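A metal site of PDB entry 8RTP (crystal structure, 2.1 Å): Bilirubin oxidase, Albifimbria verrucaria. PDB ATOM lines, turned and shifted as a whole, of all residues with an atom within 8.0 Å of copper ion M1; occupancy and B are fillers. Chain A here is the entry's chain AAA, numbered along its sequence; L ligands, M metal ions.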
ATOM      1  N   HIS A  94      -6.299  20.330 -13.804  1.00  0.00           N
ATOM      2  CA  HIS A  94      -6.347  19.454 -14.991  1.00  0.00           C
ATOM      3  C   HIS A  94      -5.749  18.077 -14.644  1.00  0.00           C
ATOM      4  O   HIS A  94      -4.525  17.989 -14.207  1.00  0.00           O
ATOM      5  CB  HIS A  94      -5.576  20.116 -16.131  1.00  0.00           C
ATOM      6  CG  HIS A  94      -5.483  19.245 -17.308  1.00  0.00           C
ATOM      7  ND1 HIS A  94      -6.599  18.617 -17.858  1.00  0.00           N
ATOM      8  CD2 HIS A  94      -4.425  18.875 -18.052  1.00  0.00           C
ATOM      9  CE1 HIS A  94      -6.231  17.939 -18.915  1.00  0.00           C
ATOM     10  NE2 HIS A  94      -4.906  18.081 -19.047  1.00  0.00           N
ATOM     11  N   LEU A  95      -6.546  17.040 -14.855  1.00  0.00           N
ATOM     12  CA  LEU A  95      -6.054  15.645 -14.900  1.00  0.00           C
ATOM     13  C   LEU A  95      -5.574  15.349 -16.312  1.00  0.00           C
ATOM     14  O   LEU A  95      -6.421  15.035 -17.156  1.00  0.00           O
ATOM     15  CB  LEU A  95      -7.179  14.678 -14.533  1.00  0.00           C
ATOM     16  CG  LEU A  95      -6.721  13.237 -14.386  1.00  0.00           C
ATOM     17  CD1 LEU A  95      -5.553  13.146 -13.390  1.00  0.00           C
ATOM     18  CD2 LEU A  95      -7.886  12.352 -13.968  1.00  0.00           C
ATOM     19  N   HIS A  96      -4.267  15.480 -16.540  1.00  0.00           N
ATOM     20  CA  HIS A  96      -3.622  15.344 -17.849  1.00  0.00           C
ATOM     21  C   HIS A  96      -3.491  13.843 -18.165  1.00  0.00           C
ATOM     22  O   HIS A  96      -2.912  13.104 -17.359  1.00  0.00           O
ATOM     23  CB  HIS A  96      -2.327  16.145 -17.813  1.00  0.00           C
ATOM     24  CG  HIS A  96      -1.639  16.204 -19.137  1.00  0.00           C
ATOM     25  ND1 HIS A  96      -0.904  17.299 -19.510  1.00  0.00           N
ATOM     26  CD2 HIS A  96      -1.514  15.314 -20.134  1.00  0.00           C
ATOM     27  CE1 HIS A  96      -0.364  17.083 -20.695  1.00  0.00           C
ATOM     28  NE2 HIS A  96      -0.723  15.864 -21.096  1.00  0.00           N
ATOM     29  N   GLY A  97      -4.076  13.438 -19.302  1.00  0.00           N
ATOM     30  CA  GLY A  97      -4.191  12.064 -19.800  1.00  0.00           C
ATOM     31  C   GLY A  97      -5.612  11.542 -19.634  1.00  0.00           C
ATOM     32  O   GLY A  97      -5.791  10.343 -19.919  1.00  0.00           O
ATOM     33  N   TRP A 132      -1.128  12.750 -14.737  1.00  0.00           N
ATOM     34  CA  TRP A 132      -0.688  13.657 -13.672  1.00  0.00           C
ATOM     35  C   TRP A 132      -1.724  14.758 -13.563  1.00  0.00           C
ATOM     36  O   TRP A 132      -2.432  15.008 -14.577  1.00  0.00           O
ATOM     37  CB  TRP A 132       0.746  14.146 -13.890  1.00  0.00           C
ATOM     38  CG  TRP A 132       1.016  14.979 -15.102  1.00  0.00           C
ATOM     39  CD1 TRP A 132       0.755  14.704 -16.415  1.00  0.00           C
ATOM     40  CD2 TRP A 132       1.662  16.263 -15.087  1.00  0.00           C
ATOM     41  NE1 TRP A 132       1.209  15.727 -17.220  1.00  0.00           N
ATOM     42  CE2 TRP A 132       1.749  16.710 -16.423  1.00  0.00           C
ATOM     43  CE3 TRP A 132       2.190  17.064 -14.077  1.00  0.00           C
ATOM     44  CZ2 TRP A 132       2.338  17.925 -16.752  1.00  0.00           C
ATOM     45  CZ3 TRP A 132       2.759  18.285 -14.416  1.00  0.00           C
ATOM     46  CH2 TRP A 132       2.856  18.684 -15.740  1.00  0.00           C
ATOM     47  N   TYR A 133      -1.931  15.237 -12.326  1.00  0.00           N
ATOM     48  CA  TYR A 133      -2.901  16.303 -12.023  1.00  0.00           C
ATOM     49  C   TYR A 133      -2.035  17.508 -11.704  1.00  0.00           C
ATOM     50  O   TYR A 133      -0.961  17.324 -11.157  1.00  0.00           O
ATOM     51  CB  TYR A 133      -3.921  15.857 -10.979  1.00  0.00           C
ATOM     52  CG  TYR A 133      -3.365  15.553  -9.613  1.00  0.00           C
ATOM     53  CD1 TYR A 133      -2.710  14.346  -9.349  1.00  0.00           C
ATOM     54  CD2 TYR A 133      -3.511  16.455  -8.578  1.00  0.00           C
ATOM     55  CE1 TYR A 133      -2.204  14.076  -8.102  1.00  0.00           C
ATOM     56  CE2 TYR A 133      -3.009  16.195  -7.318  1.00  0.00           C
ATOM     57  CZ  TYR A 133      -2.338  15.018  -7.082  1.00  0.00           C
ATOM     58  OH  TYR A 133      -1.868  14.794  -5.830  1.00  0.00           O
ATOM     59  N   HIS A 134      -2.424  18.682 -12.201  1.00  0.00           N
ATOM     60  CA  HIS A 134      -1.598  19.898 -12.041  1.00  0.00           C
ATOM     61  C   HIS A 134      -2.461  21.138 -12.251  1.00  0.00           C
ATOM     62  O   HIS A 134      -3.534  21.069 -12.916  1.00  0.00           O
ATOM     63  CB  HIS A 134      -0.363  19.834 -12.951  1.00  0.00           C
ATOM     64  CG  HIS A 134      -0.660  19.986 -14.411  1.00  0.00           C
ATOM     65  ND1 HIS A 134      -1.045  21.204 -14.967  1.00  0.00           N
ATOM     66  CD2 HIS A 134      -0.594  19.108 -15.419  1.00  0.00           C
ATOM     67  CE1 HIS A 134      -1.209  21.053 -16.259  1.00  0.00           C
ATOM     68  NE2 HIS A 134      -0.927  19.780 -16.573  1.00  0.00           N
ATOM     69  N   ASP A 135      -1.962  22.267 -11.797  1.00  0.00           N
ATOM     70  CA  ASP A 135      -2.696  23.534 -11.979  1.00  0.00           C
ATOM     71  C   ASP A 135      -2.743  23.953 -13.452  1.00  0.00           C
ATOM     72  O   ASP A 135      -1.789  23.645 -14.270  1.00  0.00           O
ATOM     73  CB  ASP A 135      -2.100  24.658 -11.148  1.00  0.00           C
ATOM     74  CG  ASP A 135      -3.112  25.774 -11.108  1.00  0.00           C
ATOM     75  OD1 ASP A 135      -4.193  25.533 -10.501  1.00  0.00           O
ATOM     76  OD2 ASP A 135      -2.832  26.834 -11.759  1.00  0.00           O
ATOM     77  N   HIS A 136      -3.810  24.652 -13.808  1.00  0.00           N
ATOM     78  CA  HIS A 136      -4.034  25.143 -15.181  1.00  0.00           C
ATOM     79  C   HIS A 136      -4.681  26.536 -15.199  1.00  0.00           C
ATOM     80  O   HIS A 136      -5.141  26.931 -16.253  1.00  0.00           O
ATOM     81  CB  HIS A 136      -4.877  24.095 -15.889  1.00  0.00           C
ATOM     82  CG  HIS A 136      -4.556  23.952 -17.326  1.00  0.00           C
ATOM     83  ND1 HIS A 136      -4.626  25.023 -18.191  1.00  0.00           N
ATOM     84  CD2 HIS A 136      -4.192  22.861 -18.050  1.00  0.00           C
ATOM     85  CE1 HIS A 136      -4.280  24.612 -19.402  1.00  0.00           C
ATOM     86  NE2 HIS A 136      -4.038  23.280 -19.343  1.00  0.00           N
ATOM     87  N   THR A 141      -0.496  29.442 -14.401  1.00  0.00           N
ATOM     88  CA  THR A 141      -0.177  27.986 -14.450  1.00  0.00           C
ATOM     89  C   THR A 141       1.312  27.753 -14.150  1.00  0.00           C
ATOM     90  O   THR A 141       1.639  26.831 -13.381  1.00  0.00           O
ATOM     91  CB  THR A 141      -0.607  27.376 -15.796  1.00  0.00           C
ATOM     92  OG1 THR A 141      -2.024  27.441 -15.833  1.00  0.00           O
ATOM     93  CG2 THR A 141      -0.166  25.941 -15.983  1.00  0.00           C
ATOM     94  N   LEU A 226       8.162  11.674 -15.829  1.00  0.00           N
ATOM     95  CA  LEU A 226       7.253  12.820 -16.126  1.00  0.00           C
ATOM     96  C   LEU A 226       8.098  14.094 -16.126  1.00  0.00           C
ATOM     97  O   LEU A 226       8.884  14.281 -15.168  1.00  0.00           O
ATOM     98  CB  LEU A 226       6.176  12.897 -15.047  1.00  0.00           C
ATOM     99  CG  LEU A 226       5.416  14.225 -14.986  1.00  0.00           C
ATOM    100  CD1 LEU A 226       4.657  14.504 -16.278  1.00  0.00           C
ATOM    101  CD2 LEU A 226       4.457  14.223 -13.815  1.00  0.00           C
ATOM    102  N   ASP A 227       8.050  14.865 -17.202  1.00  0.00           N
ATOM    103  CA  ASP A 227       8.734  16.181 -17.219  1.00  0.00           C
ATOM    104  C   ASP A 227       7.688  17.167 -16.700  1.00  0.00           C
ATOM    105  O   ASP A 227       6.773  17.581 -17.461  1.00  0.00           O
ATOM    106  CB  ASP A 227       9.374  16.504 -18.579  1.00  0.00           C
ATOM    107  CG  ASP A 227      10.034  17.869 -18.575  1.00  0.00           C
ATOM    108  OD1 ASP A 227       9.985  18.541 -17.519  1.00  0.00           O
ATOM    109  OD2 ASP A 227      10.683  18.199 -19.559  1.00  0.00           O
ATOM    110  N   MET A 273       8.145  18.904 -21.771  1.00  0.00           N
ATOM    111  CA  MET A 273       7.143  19.258 -20.742  1.00  0.00           C
ATOM    112  C   MET A 273       5.843  18.515 -21.007  1.00  0.00           C
ATOM    113  O   MET A 273       5.246  18.656 -22.130  1.00  0.00           O
ATOM    114  CB  MET A 273       6.903  20.782 -20.700  1.00  0.00           C
ATOM    115  CG  MET A 273       8.090  21.558 -20.163  1.00  0.00           C
ATOM    116  SD  MET A 273       9.492  21.695 -21.274  1.00  0.00           S
ATOM    117  CE  MET A 273       8.926  22.972 -22.392  1.00  0.00           C
ATOM    118  N   ALA A 274       5.401  17.798 -19.978  1.00  0.00           N
ATOM    119  CA  ALA A 274       4.097  17.118 -19.794  1.00  0.00           C
ATOM    120  C   ALA A 274       4.126  15.719 -20.402  1.00  0.00           C
ATOM    121  O   ALA A 274       3.122  15.017 -20.265  1.00  0.00           O
ATOM    122  CB  ALA A 274       2.956  17.921 -20.351  1.00  0.00           C
ATOM    123  N   GLU A 275       5.194  15.327 -21.063  1.00  0.00           N
ATOM    124  CA  GLU A 275       5.295  13.968 -21.654  1.00  0.00           C
ATOM    125  C   GLU A 275       5.577  12.986 -20.522  1.00  0.00           C
ATOM    126  O   GLU A 275       6.300  13.350 -19.537  1.00  0.00           O
ATOM    127  CB  GLU A 275       6.380  13.873 -22.724  1.00  0.00           C
ATOM    128  CG  GLU A 275       6.095  14.596 -24.031  1.00  0.00           C
ATOM    129  CD  GLU A 275       7.123  14.312 -25.104  1.00  0.00           C
ATOM    130  OE1 GLU A 275       8.353  14.429 -24.854  1.00  0.00           O
ATOM    131  OE2 GLU A 275       6.700  13.930 -26.185  1.00  0.00           O
ATOM    132  N   ARG A 276       4.987  11.802 -20.606  1.00  0.00           N
ATOM    133  CA  ARG A 276       5.264  10.668 -19.679  1.00  0.00           C
ATOM    134  C   ARG A 276       5.781   9.529 -20.552  1.00  0.00           C
ATOM    135  O   ARG A 276       5.193   9.232 -21.619  1.00  0.00           O
ATOM    136  CB  ARG A 276       4.044  10.155 -18.903  1.00  0.00           C
ATOM    137  CG  ARG A 276       3.518  11.118 -17.845  1.00  0.00           C
ATOM    138  CD  ARG A 276       2.674  12.217 -18.502  1.00  0.00           C
ATOM    139  NE  ARG A 276       1.389  11.711 -18.954  1.00  0.00           N
ATOM    140  CZ  ARG A 276       0.673  12.193 -19.966  1.00  0.00           C
ATOM    141  NH1 ARG A 276      -0.490  11.645 -20.250  1.00  0.00           N
ATOM    142  NH2 ARG A 276       1.115  13.221 -20.702  1.00  0.00           N
ATOM    143  N   HIS A 401       0.275  20.075 -26.370  1.00  0.00           N
ATOM    144  CA  HIS A 401      -0.720  19.223 -25.694  1.00  0.00           C
ATOM    145  C   HIS A 401      -2.109  19.515 -26.247  1.00  0.00           C
ATOM    146  O   HIS A 401      -2.520  20.712 -26.361  1.00  0.00           O
ATOM    147  CB  HIS A 401      -0.563  19.435 -24.185  1.00  0.00           C
ATOM    148  CG  HIS A 401      -1.587  18.668 -23.442  1.00  0.00           C
ATOM    149  ND1 HIS A 401      -1.913  17.368 -23.767  1.00  0.00           N
ATOM    150  CD2 HIS A 401      -2.397  19.029 -22.438  1.00  0.00           C
ATOM    151  CE1 HIS A 401      -2.861  16.958 -22.965  1.00  0.00           C
ATOM    152  NE2 HIS A 401      -3.179  17.962 -22.148  1.00  0.00           N
ATOM    153  N   HIS A 403      -5.895  18.479 -25.276  1.00  0.00           N
ATOM    154  CA  HIS A 403      -6.861  17.921 -24.301  1.00  0.00           C
ATOM    155  C   HIS A 403      -7.831  16.970 -25.010  1.00  0.00           C
ATOM    156  O   HIS A 403      -7.901  17.027 -26.243  1.00  0.00           O
ATOM    157  CB  HIS A 403      -7.577  19.079 -23.637  1.00  0.00           C
ATOM    158  CG  HIS A 403      -6.757  19.781 -22.618  1.00  0.00           C
ATOM    159  ND1 HIS A 403      -7.192  19.928 -21.323  1.00  0.00           N
ATOM    160  CD2 HIS A 403      -5.585  20.465 -22.710  1.00  0.00           C
ATOM    161  CE1 HIS A 403      -6.293  20.617 -20.643  1.00  0.00           C
ATOM    162  NE2 HIS A 403      -5.321  20.977 -21.465  1.00  0.00           N
ATOM    163  N   ASP A 430      -0.266  12.410 -25.928  1.00  0.00           N
ATOM    164  CA  ASP A 430      -1.190  13.580 -25.848  1.00  0.00           C
ATOM    165  C   ASP A 430      -0.356  14.855 -25.828  1.00  0.00           C
ATOM    166  O   ASP A 430      -0.932  15.971 -25.763  1.00  0.00           O
ATOM    167  CB  ASP A 430      -2.175  13.443 -24.685  1.00  0.00           C
ATOM    168  CG  ASP A 430      -1.548  13.258 -23.316  1.00  0.00           C
ATOM    169  OD1 ASP A 430      -0.471  13.862 -23.080  1.00  0.00           O
ATOM    170  OD2 ASP A 430      -2.197  12.540 -22.475  1.00  0.00           O
ATOM    171  N   VAL A 431       0.953  14.697 -25.897  1.00  0.00           N
ATOM    172  CA  VAL A 431       1.947  15.795 -26.008  1.00  0.00           C
ATOM    173  C   VAL A 431       2.980  15.402 -27.065  1.00  0.00           C
ATOM    174  O   VAL A 431       3.409  14.208 -27.150  1.00  0.00           O
ATOM    175  CB  VAL A 431       2.629  16.059 -24.657  1.00  0.00           C
ATOM    176  CG1 VAL A 431       3.682  17.120 -24.791  1.00  0.00           C
ATOM    177  CG2 VAL A 431       1.623  16.465 -23.597  1.00  0.00           C
ATOM    178  N   HIS A 456      -2.474  23.594 -26.494  1.00  0.00           N
ATOM    179  CA  HIS A 456      -1.476  24.616 -26.139  1.00  0.00           C
ATOM    180  C   HIS A 456      -0.089  24.010 -26.123  1.00  0.00           C
ATOM    181  O   HIS A 456       0.082  22.721 -26.059  1.00  0.00           O
ATOM    182  CB  HIS A 456      -1.841  25.212 -24.773  1.00  0.00           C
ATOM    183  CG  HIS A 456      -1.913  24.208 -23.672  1.00  0.00           C
ATOM    184  ND1 HIS A 456      -0.819  23.928 -22.875  1.00  0.00           N
ATOM    185  CD2 HIS A 456      -2.934  23.453 -23.217  1.00  0.00           C
ATOM    186  CE1 HIS A 456      -1.151  23.028 -21.979  1.00  0.00           C
ATOM    187  NE2 HIS A 456      -2.444  22.707 -22.174  1.00  0.00           N
ATOM    188  N   HIS A 458       3.050  23.343 -23.773  1.00  0.00           N
ATOM    189  CA  HIS A 458       3.180  22.957 -22.353  1.00  0.00           C
ATOM    190  C   HIS A 458       4.465  23.513 -21.811  1.00  0.00           C
ATOM    191  O   HIS A 458       4.818  23.188 -20.644  1.00  0.00           O
ATOM    192  CB  HIS A 458       3.074  21.427 -22.175  1.00  0.00           C
ATOM    193  CG  HIS A 458       2.336  21.039 -20.957  1.00  0.00           C
ATOM    194  ND1 HIS A 458       2.798  21.322 -19.689  1.00  0.00           N
ATOM    195  CD2 HIS A 458       1.123  20.468 -20.795  1.00  0.00           C
ATOM    196  CE1 HIS A 458       1.931  20.889 -18.792  1.00  0.00           C
ATOM    197  NE2 HIS A 458       0.883  20.379 -19.448  1.00  0.00           N
ATOM    198  N   LEU A 460       5.197  26.187 -19.821  1.00  0.00           N
ATOM    199  CA  LEU A 460       4.214  26.901 -18.954  1.00  0.00           C
ATOM    200  C   LEU A 460       4.380  28.434 -19.064  1.00  0.00           C
ATOM    201  O   LEU A 460       3.355  29.137 -18.894  1.00  0.00           O
ATOM    202  CB  LEU A 460       4.326  26.404 -17.514  1.00  0.00           C
ATOM    203  CG  LEU A 460       4.101  24.905 -17.295  1.00  0.00           C
ATOM    204  CD1 LEU A 460       4.080  24.620 -15.822  1.00  0.00           C
ATOM    205  CD2 LEU A 460       2.821  24.391 -17.947  1.00  0.00           C
ATOM    206  N   GLU A 463       2.625  29.005 -22.410  1.00  0.00           N
ATOM    207  CA  GLU A 463       1.226  28.709 -22.114  1.00  0.00           C
ATOM    208  C   GLU A 463       0.539  29.945 -21.508  1.00  0.00           C
ATOM    209  O   GLU A 463      -0.569  30.309 -21.939  1.00  0.00           O
ATOM    210  CB  GLU A 463       1.173  27.544 -21.134  1.00  0.00           C
ATOM    211  CG  GLU A 463      -0.239  27.107 -20.829  1.00  0.00           C
ATOM    212  CD  GLU A 463      -0.405  25.762 -20.122  1.00  0.00           C
ATOM    213  OE1 GLU A 463       0.524  24.901 -20.246  1.00  0.00           O
ATOM    214  OE2 GLU A 463      -1.445  25.617 -19.400  1.00  0.00           O
HETATM  215  O1  LIG L   1      -2.479  20.567 -20.000  1.00  0.00           O
HETATM  216  O2  LIG L   1      -1.870  21.253 -19.226  1.00  0.00           O
HETATM  217 CU    CU M   1      -0.618  19.048 -18.456  1.00  0.00          CU
HETATM  218 CU    CU M   2      -3.985  18.045 -20.567  1.00  0.00          CU
HETATM  219 CU    CU M   3      -3.741  21.992 -20.777  1.00  0.00          CU
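A ring nitrogen (NE2) of His 134 is bound to copper ion M1 (2.0 Å).
A ring nitrogen (ND1) of His 96 is bound to copper ion M1 (2.1 Å).
Copper ion M1 is bound by NE2 of His 458, at 2.2 Å.
Slightly farther from copper ion M1 lies an oxygen (O2) of the ligand (2.6 Å).
NH2 of Arg 276 is in hydrogen-bond range of NE2 of His 96 (3.2 Å).
N of His 134 lies within hydrogen-bond range of O of His 94.
N of His 96 is in hydrogen-bond range of O of Trp 132 (2.7 Å).
NE2 of His 96 is in hydrogen-bond range of OD1 of Asp 430, 2.8 Å away.
A ring nitrogen (NE2) of His 96 lies close to a ring nitrogen (ND1) of His 401.
His 94 touches copper ion M1 (CD2 to CU, 3.8 Å).
CZ2 of Trp 132 touches copper ion M1, at 3.6 Å.
Five residues have an atom within 4 Å of copper ion M1: His 94, His 96, Trp 132, His 134 and His 458.
The nearest printed residue that does not touch copper ion M1 is Ala 274 (4.2 Å).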
